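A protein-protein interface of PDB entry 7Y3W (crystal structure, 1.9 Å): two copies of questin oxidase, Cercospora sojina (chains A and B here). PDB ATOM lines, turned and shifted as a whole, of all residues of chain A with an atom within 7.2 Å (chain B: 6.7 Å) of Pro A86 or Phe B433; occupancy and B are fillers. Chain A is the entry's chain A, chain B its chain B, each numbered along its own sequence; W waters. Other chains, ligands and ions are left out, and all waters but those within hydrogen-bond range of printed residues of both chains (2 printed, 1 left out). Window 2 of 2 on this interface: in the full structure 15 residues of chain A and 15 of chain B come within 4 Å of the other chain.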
ATOM      1  N   ASP A  41     -23.500  10.613  10.532  1.00  0.00           N
ATOM      2  CA  ASP A  41     -22.953  11.842   9.921  1.00  0.00           C
ATOM      3  C   ASP A  41     -21.423  11.807   9.857  1.00  0.00           C
ATOM      4  O   ASP A  41     -20.870  12.237   8.849  1.00  0.00           O
ATOM      5  CB  ASP A  41     -23.406  13.057  10.725  1.00  0.00           C
ATOM      6  CG  ASP A  41     -24.881  13.401  10.585  1.00  0.00           C
ATOM      7  OD1 ASP A  41     -25.538  12.818   9.728  1.00  0.00           O
ATOM      8  OD2 ASP A  41     -25.341  14.245  11.359  1.00  0.00           O
ATOM      9  N   GLU A  42     -20.757  11.311  10.888  1.00  0.00           N
ATOM     10  CA  GLU A  42     -19.305  11.569  11.070  1.00  0.00           C
ATOM     11  C   GLU A  42     -18.458  10.399  10.567  1.00  0.00           C
ATOM     12  O   GLU A  42     -17.270  10.649  10.227  1.00  0.00           O
ATOM     13  CB  GLU A  42     -19.013  11.833  12.547  1.00  0.00           C
ATOM     14  CG  GLU A  42     -19.635  13.109  13.076  1.00  0.00           C
ATOM     15  CD  GLU A  42     -19.595  13.232  14.598  1.00  0.00           C
ATOM     16  OE1 GLU A  42     -18.598  12.745  15.199  1.00  0.00           O
ATOM     17  OE2 GLU A  42     -20.583  13.786  15.195  1.00  0.00           O
ATOM     18  N   PHE A  43     -18.971   9.162  10.633  1.00  0.00           N
ATOM     19  CA  PHE A  43     -18.117   7.955  10.546  1.00  0.00           C
ATOM     20  C   PHE A  43     -18.401   7.105   9.315  1.00  0.00           C
ATOM     21  O   PHE A  43     -19.574   6.921   8.885  1.00  0.00           O
ATOM     22  CB  PHE A  43     -18.209   7.165  11.850  1.00  0.00           C
ATOM     23  CG  PHE A  43     -17.845   7.981  13.062  1.00  0.00           C
ATOM     24  CD1 PHE A  43     -16.706   8.790  13.067  1.00  0.00           C
ATOM     25  CD2 PHE A  43     -18.609   7.914  14.221  1.00  0.00           C
ATOM     26  CE1 PHE A  43     -16.392   9.568  14.179  1.00  0.00           C
ATOM     27  CE2 PHE A  43     -18.293   8.705  15.320  1.00  0.00           C
ATOM     28  CZ  PHE A  43     -17.185   9.519  15.308  1.00  0.00           C
ATOM     29  N   ASP A  44     -17.316   6.530   8.790  1.00  0.00           N
ATOM     30  CA  ASP A  44     -17.366   5.545   7.688  1.00  0.00           C
ATOM     31  C   ASP A  44     -17.986   4.227   8.184  1.00  0.00           C
ATOM     32  O   ASP A  44     -18.137   3.986   9.379  1.00  0.00           O
ATOM     33  CB  ASP A  44     -16.004   5.347   7.032  1.00  0.00           C
ATOM     34  CG  ASP A  44     -16.186   5.052   5.547  1.00  0.00           C
ATOM     35  OD1 ASP A  44     -16.284   6.021   4.756  1.00  0.00           O
ATOM     36  OD2 ASP A  44     -16.344   3.882   5.199  1.00  0.00           O
ATOM     37  N   MET A  45     -18.374   3.385   7.234  1.00  0.00           N
ATOM     38  CA  MET A  45     -18.838   2.056   7.548  1.00  0.00           C
ATOM     39  C   MET A  45     -17.625   1.140   7.760  1.00  0.00           C
ATOM     40  O   MET A  45     -17.757   0.090   8.349  1.00  0.00           O
ATOM     41  CB  MET A  45     -19.814   1.607   6.454  1.00  0.00           C
ATOM     42  CG  MET A  45     -20.454   0.248   6.653  1.00  0.00           C
ATOM     43  SD  MET A  45     -21.610   0.357   8.265  1.00  0.00           S
ATOM     44  CE  MET A  45     -22.902   1.709   7.681  1.00  0.00           C
ATOM     45  N   PHE A  46     -16.451   1.503   7.259  1.00  0.00           N
ATOM     46  CA  PHE A  46     -15.331   0.574   7.247  1.00  0.00           C
ATOM     47  C   PHE A  46     -14.092   1.274   7.789  1.00  0.00           C
ATOM     48  O   PHE A  46     -13.683   2.361   7.281  1.00  0.00           O
ATOM     49  CB  PHE A  46     -15.038   0.034   5.837  1.00  0.00           C
ATOM     50  CG  PHE A  46     -16.225  -0.597   5.164  1.00  0.00           C
ATOM     51  CD1 PHE A  46     -16.690  -1.840   5.549  1.00  0.00           C
ATOM     52  CD2 PHE A  46     -16.874   0.046   4.121  1.00  0.00           C
ATOM     53  CE1 PHE A  46     -17.811  -2.386   4.945  1.00  0.00           C
ATOM     54  CE2 PHE A  46     -17.997  -0.509   3.521  1.00  0.00           C
ATOM     55  CZ  PHE A  46     -18.428  -1.755   3.909  1.00  0.00           C
ATOM     56  N   ASP A  81     -15.291   3.339  19.878  1.00  0.00           N
ATOM     57  CA  ASP A  81     -14.362   4.393  19.381  1.00  0.00           C
ATOM     58  C   ASP A  81     -13.407   3.806  18.327  1.00  0.00           C
ATOM     59  O   ASP A  81     -13.160   4.484  17.347  1.00  0.00           O
ATOM     60  CB  ASP A  81     -13.621   5.076  20.527  1.00  0.00           C
ATOM     61  CG  ASP A  81     -12.753   6.244  20.081  1.00  0.00           C
ATOM     62  OD1 ASP A  81     -13.270   7.318  19.924  1.00  0.00           O
ATOM     63  OD2 ASP A  81     -11.594   6.036  19.865  1.00  0.00           O
ATOM     64  N   PRO A  82     -12.832   2.574  18.472  1.00  0.00           N
ATOM     65  CA  PRO A  82     -11.936   2.022  17.448  1.00  0.00           C
ATOM     66  C   PRO A  82     -12.616   1.822  16.086  1.00  0.00           C
ATOM     67  O   PRO A  82     -11.936   1.846  15.092  1.00  0.00           O
ATOM     68  CB  PRO A  82     -11.428   0.697  18.061  1.00  0.00           C
ATOM     69  CG  PRO A  82     -11.622   0.887  19.562  1.00  0.00           C
ATOM     70  CD  PRO A  82     -12.879   1.717  19.670  1.00  0.00           C
ATOM     71  N   GLN A  84     -14.716   3.911  14.717  1.00  0.00           N
ATOM     72  CA  GLN A  84     -15.222   5.243  14.312  1.00  0.00           C
ATOM     73  C   GLN A  84     -14.094   6.045  13.650  1.00  0.00           C
ATOM     74  O   GLN A  84     -13.327   6.684  14.348  1.00  0.00           O
ATOM     75  CB  GLN A  84     -15.802   5.970  15.528  1.00  0.00           C
ATOM     76  CG  GLN A  84     -17.079   5.309  16.039  1.00  0.00           C
ATOM     77  CD  GLN A  84     -17.511   5.715  17.422  1.00  0.00           C
ATOM     78  OE1 GLN A  84     -16.907   6.582  18.055  1.00  0.00           O
ATOM     79  NE2 GLN A  84     -18.543   5.055  17.931  1.00  0.00           N
ATOM     80  N   VAL A  85     -14.067   6.072  12.326  1.00  0.00           N
ATOM     81  CA  VAL A  85     -13.076   6.874  11.574  1.00  0.00           C
ATOM     82  C   VAL A  85     -13.829   7.793  10.632  1.00  0.00           C
ATOM     83  O   VAL A  85     -14.967   7.506  10.262  1.00  0.00           O
ATOM     84  CB  VAL A  85     -12.083   5.982  10.823  1.00  0.00           C
ATOM     85  CG1 VAL A  85     -11.360   5.075  11.786  1.00  0.00           C
ATOM     86  CG2 VAL A  85     -12.742   5.198   9.708  1.00  0.00           C
ATOM     87  N   PRO A  86     -13.211   8.916  10.213  1.00  0.00           N
ATOM     88  CA  PRO A  86     -13.912   9.914   9.405  1.00  0.00           C
ATOM     89  C   PRO A  86     -14.535   9.322   8.135  1.00  0.00           C
ATOM     90  O   PRO A  86     -13.882   8.566   7.409  1.00  0.00           O
ATOM     91  CB  PRO A  86     -12.821  10.958   9.117  1.00  0.00           C
ATOM     92  CG  PRO A  86     -11.904  10.818  10.285  1.00  0.00           C
ATOM     93  CD  PRO A  86     -11.841   9.322  10.535  1.00  0.00           C
ATOM     94  N   ILE A  87     -15.823   9.620   7.910  1.00  0.00           N
ATOM     95  CA  ILE A  87     -16.548   9.210   6.664  1.00  0.00           C
ATOM     96  C   ILE A  87     -15.819   9.778   5.435  1.00  0.00           C
ATOM     97  O   ILE A  87     -15.345  10.953   5.451  1.00  0.00           O
ATOM     98  CB  ILE A  87     -18.038   9.617   6.712  1.00  0.00           C
ATOM     99  CG1 ILE A  87     -18.837   9.024   5.548  1.00  0.00           C
ATOM    100  CG2 ILE A  87     -18.238  11.141   6.797  1.00  0.00           C
ATOM    101  CD1 ILE A  87     -20.340   9.012   5.802  1.00  0.00           C
ATOM    102  N   GLY A  88     -15.703   8.977   4.391  1.00  0.00           N
ATOM    103  CA  GLY A  88     -15.108   9.418   3.120  1.00  0.00           C
ATOM    104  C   GLY A  88     -15.864  10.587   2.501  1.00  0.00           C
ATOM    105  O   GLY A  88     -17.123  10.678   2.614  1.00  0.00           O
ATOM    106  N   ALA A  89     -15.121  11.477   1.851  1.00  0.00           N
ATOM    107  CA  ALA A  89     -15.654  12.595   1.044  1.00  0.00           C
ATOM    108  C   ALA A  89     -16.571  12.006  -0.025  1.00  0.00           C
ATOM    109  O   ALA A  89     -16.259  10.922  -0.538  1.00  0.00           O
ATOM    110  CB  ALA A  89     -14.508  13.384   0.441  1.00  0.00           C
ATOM    111  N   MET B 230      -5.759   6.259   4.635  1.00  0.00           N
ATOM    112  CA  MET B 230      -5.537   5.840   5.997  1.00  0.00           C
ATOM    113  C   MET B 230      -6.119   4.446   6.243  1.00  0.00           C
ATOM    114  O   MET B 230      -5.428   3.591   6.789  1.00  0.00           O
ATOM    115  CB  MET B 230      -6.166   6.794   7.007  1.00  0.00           C
ATOM    116  CG  MET B 230      -5.833   6.390   8.424  1.00  0.00           C
ATOM    117  SD  MET B 230      -6.672   7.608   9.694  1.00  0.00           S
ATOM    118  CE  MET B 230      -8.520   6.864   9.726  1.00  0.00           C
ATOM    119  N   THR B 231      -7.377   4.226   5.849  1.00  0.00           N
ATOM    120  CA  THR B 231      -8.053   2.959   6.155  1.00  0.00           C
ATOM    121  C   THR B 231      -7.670   1.839   5.178  1.00  0.00           C
ATOM    122  O   THR B 231      -8.247   0.720   5.269  1.00  0.00           O
ATOM    123  CB  THR B 231      -9.577   3.122   6.219  1.00  0.00           C
ATOM    124  OG1 THR B 231     -10.049   3.577   4.955  1.00  0.00           O
ATOM    125  CG2 THR B 231      -9.985   4.083   7.313  1.00  0.00           C
ATOM    126  N   ARG B 283       4.107  16.683  15.790  1.00  0.00           N
ATOM    127  CA  ARG B 283       3.002  17.676  15.678  1.00  0.00           C
ATOM    128  C   ARG B 283       3.068  18.643  16.867  1.00  0.00           C
ATOM    129  O   ARG B 283       3.302  18.253  18.006  1.00  0.00           O
ATOM    130  CB  ARG B 283       1.627  17.003  15.668  1.00  0.00           C
ATOM    131  CG  ARG B 283       1.366  16.062  14.498  1.00  0.00           C
ATOM    132  CD  ARG B 283       1.257  16.772  13.167  1.00  0.00           C
ATOM    133  NE  ARG B 283       0.903  15.868  12.087  1.00  0.00           N
ATOM    134  CZ  ARG B 283      -0.270  15.831  11.462  1.00  0.00           C
ATOM    135  NH1 ARG B 283      -1.263  16.639  11.822  1.00  0.00           N
ATOM    136  NH2 ARG B 283      -0.472  14.924  10.514  1.00  0.00           N
ATOM    137  N   GLY B 430       1.458  11.031   8.917  1.00  0.00           N
ATOM    138  CA  GLY B 430       0.868  12.084   8.068  1.00  0.00           C
ATOM    139  C   GLY B 430      -0.647  12.148   8.189  1.00  0.00           C
ATOM    140  O   GLY B 430      -1.242  13.107   7.652  1.00  0.00           O
ATOM    141  N   TYR B 431      -1.298  11.142   8.777  1.00  0.00           N
ATOM    142  CA  TYR B 431      -2.782  11.085   8.834  1.00  0.00           C
ATOM    143  C   TYR B 431      -3.242  11.860  10.082  1.00  0.00           C
ATOM    144  O   TYR B 431      -3.029  11.385  11.191  1.00  0.00           O
ATOM    145  CB  TYR B 431      -3.295   9.644   8.828  1.00  0.00           C
ATOM    146  CG  TYR B 431      -2.944   8.896   7.589  1.00  0.00           C
ATOM    147  CD1 TYR B 431      -3.532   9.236   6.378  1.00  0.00           C
ATOM    148  CD2 TYR B 431      -2.020   7.876   7.615  1.00  0.00           C
ATOM    149  CE1 TYR B 431      -3.218   8.561   5.211  1.00  0.00           C
ATOM    150  CE2 TYR B 431      -1.667   7.217   6.452  1.00  0.00           C
ATOM    151  CZ  TYR B 431      -2.275   7.551   5.250  1.00  0.00           C
ATOM    152  OH  TYR B 431      -1.938   6.893   4.106  1.00  0.00           O
ATOM    153  N   ASP B 432      -3.797  13.066   9.890  1.00  0.00           N
ATOM    154  CA  ASP B 432      -4.249  13.966  10.993  1.00  0.00           C
ATOM    155  C   ASP B 432      -5.072  13.171  12.014  1.00  0.00           C
ATOM    156  O   ASP B 432      -4.877  13.312  13.217  1.00  0.00           O
ATOM    157  CB  ASP B 432      -5.078  15.147  10.459  1.00  0.00           C
ATOM    158  CG  ASP B 432      -4.266  16.125   9.633  1.00  0.00           C
ATOM    159  OD1 ASP B 432      -3.054  16.057   9.708  1.00  0.00           O
ATOM    160  OD2 ASP B 432      -4.874  16.859   8.841  1.00  0.00           O
ATOM    161  N   PHE B 433      -5.989  12.348  11.555  1.00  0.00           N
ATOM    162  CA  PHE B 433      -6.912  11.649  12.470  1.00  0.00           C
ATOM    163  C   PHE B 433      -6.156  10.805  13.492  1.00  0.00           C
ATOM    164  O   PHE B 433      -6.608  10.799  14.623  1.00  0.00           O
ATOM    165  CB  PHE B 433      -7.921  10.824  11.689  1.00  0.00           C
ATOM    166  CG  PHE B 433      -8.848  10.050  12.588  1.00  0.00           C
ATOM    167  CD1 PHE B 433      -9.949  10.672  13.160  1.00  0.00           C
ATOM    168  CD2 PHE B 433      -8.595   8.719  12.879  1.00  0.00           C
ATOM    169  CE1 PHE B 433     -10.813   9.954  13.984  1.00  0.00           C
ATOM    170  CE2 PHE B 433      -9.441   8.008  13.715  1.00  0.00           C
ATOM    171  CZ  PHE B 433     -10.549   8.634  14.269  1.00  0.00           C
ATOM    172  N   LEU B 434      -5.038  10.150  13.135  1.00  0.00           N
ATOM    173  CA  LEU B 434      -4.339   9.263  14.100  1.00  0.00           C
ATOM    174  C   LEU B 434      -3.806  10.081  15.270  1.00  0.00           C
ATOM    175  O   LEU B 434      -3.690   9.516  16.391  1.00  0.00           O
ATOM    176  CB  LEU B 434      -3.231   8.494  13.393  1.00  0.00           C
ATOM    177  CG  LEU B 434      -3.738   7.509  12.346  1.00  0.00           C
ATOM    178  CD1 LEU B 434      -2.584   6.698  11.756  1.00  0.00           C
ATOM    179  CD2 LEU B 434      -4.785   6.571  12.935  1.00  0.00           C
ATOM    180  N   TRP B 435      -3.502  11.362  15.050  1.00  0.00           N
ATOM    181  CA  TRP B 435      -3.003  12.244  16.133  1.00  0.00           C
ATOM    182  C   TRP B 435      -4.128  12.621  17.095  1.00  0.00           C
ATOM    183  O   TRP B 435      -3.800  13.013  18.263  1.00  0.00           O
ATOM    184  CB  TRP B 435      -2.302  13.473  15.576  1.00  0.00           C
ATOM    185  CG  TRP B 435      -0.991  13.117  14.974  1.00  0.00           C
ATOM    186  CD1 TRP B 435      -0.767  12.869  13.654  1.00  0.00           C
ATOM    187  CD2 TRP B 435       0.264  12.919  15.654  1.00  0.00           C
ATOM    188  NE1 TRP B 435       0.550  12.596  13.459  1.00  0.00           N
ATOM    189  CE2 TRP B 435       1.208  12.622  14.656  1.00  0.00           C
ATOM    190  CE3 TRP B 435       0.681  12.996  16.984  1.00  0.00           C
ATOM    191  CZ2 TRP B 435       2.538  12.347  14.949  1.00  0.00           C
ATOM    192  CZ3 TRP B 435       1.997  12.748  17.276  1.00  0.00           C
ATOM    193  CH2 TRP B 435       2.913  12.429  16.268  1.00  0.00           C
ATOM    194  N   THR B 436      -5.407  12.461  16.713  1.00  0.00           N
ATOM    195  CA  THR B 436      -6.498  12.745  17.683  1.00  0.00           C
ATOM    196  C   THR B 436      -6.504  11.659  18.751  1.00  0.00           C
ATOM    197  O   THR B 436      -7.137  11.869  19.800  1.00  0.00           O
ATOM    198  CB  THR B 436      -7.888  12.899  17.057  1.00  0.00           C
ATOM    199  OG1 THR B 436      -8.317  11.624  16.582  1.00  0.00           O
ATOM    200  CG2 THR B 436      -7.897  13.974  15.993  1.00  0.00           C
ATOM    201  N   ARG B 437      -5.824  10.534  18.527  1.00  0.00           N
ATOM    202  CA  ARG B 437      -5.773   9.442  19.533  1.00  0.00           C
ATOM    203  C   ARG B 437      -4.466   9.541  20.307  1.00  0.00           C
ATOM    204  O   ARG B 437      -4.190   8.634  21.074  1.00  0.00           O
ATOM    205  CB  ARG B 437      -5.934   8.061  18.877  1.00  0.00           C
ATOM    206  CG  ARG B 437      -7.304   7.879  18.246  1.00  0.00           C
ATOM    207  CD  ARG B 437      -7.483   6.595  17.475  1.00  0.00           C
ATOM    208  NE  ARG B 437      -8.880   6.442  17.086  1.00  0.00           N
ATOM    209  CZ  ARG B 437      -9.327   5.500  16.266  1.00  0.00           C
ATOM    210  NH1 ARG B 437      -8.474   4.639  15.744  1.00  0.00           N
ATOM    211  NH2 ARG B 437     -10.604   5.440  15.929  1.00  0.00           N
ATOM    212  N   VAL B 438      -3.664  10.573  20.094  1.00  0.00           N
ATOM    213  CA  VAL B 438      -2.354  10.672  20.792  1.00  0.00           C
ATOM    214  C   VAL B 438      -2.498  11.719  21.898  1.00  0.00           C
ATOM    215  O   VAL B 438      -3.250  12.674  21.654  1.00  0.00           O
ATOM    216  CB  VAL B 438      -1.251  10.986  19.775  1.00  0.00           C
ATOM    217  CG1 VAL B 438       0.046  11.455  20.418  1.00  0.00           C
ATOM    218  CG2 VAL B 438      -1.028   9.763  18.888  1.00  0.00           C
HETATM  219  O   HOH W   1     -12.531   2.346   4.642  1.00  0.00           O
HETATM  220  O   HOH W   2     -11.074   8.161  17.852  1.00  0.00           O
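Water W1 bridges the side-chain hydroxyl of Thr B231 (2.8 Å) and the backbone carbonyl oxygen of Phe A46 (2.9 Å).
Water W2 bridges NE of Arg B437 and OD2 of Asp A81.
The backbone carbonyl oxygen of Val A85 lies within hydrogen-bond range of the backbone NH of Asp A44 (2.9 Å).
The side-chain hydroxyl (OG1) of Thr B436 sits at hydrogen-bond distance from the backbone carbonyl oxygen (O) of Phe B433 (2.7 Å).
No position is printed for both chains.
NH2 of Arg B437 sits at hydrogen-bond distance from O of Gln A84 (3.4 Å).
OD2 of Asp A81 lies within salt-bridge range of NE of Arg B437.
Arg B437 touches Pro A82 (NH2 to O, 3.9 Å).
Phe B433 touches Gln A84.
Val A85 touches Met B230.
Thr B231 touches Val A85 (CG2 to CG2, 3.8 Å).
Pro A86 touches Phe B433 (CG to CD1, 3.5 Å).
Of the printed residues of chain B, Gln A84 touches Phe B433 (3.4 Å) and Arg B437 (3.4 Å).
Of chain B, only Phe B433 comes within 4 Å of Pro A86.
Of the printed residues of chain A, Thr B231 touches Val A85.
Of the printed residues of chain A, Phe B433 touches Gln A84 and Pro A86.
Leu B434 touches none of the printed residues of chain A.
The nearest printed residue of chain A that does not touch Phe B433 is Val A85 (4.001 Å).
Of the 14 printed residues of chain A, 5 touch a printed residue of chain B.
Along chain A the printed residues that touch a printed residue of chain B span positions 81 to 86.
Of the 12 printed residues of chain B, 4 touch a printed residue of chain A.
Along chain B the printed residues that touch a printed residue of chain A span positions 230 to 437.
Among the printed residues, 7 pairs touch across the chains.
Among the printed residues, Asp or Glu carboxylates within 4 Å of a Lys or Arg side-chain nitrogen of the other chain: Asp A81 with Arg B437 (3.9 Å).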
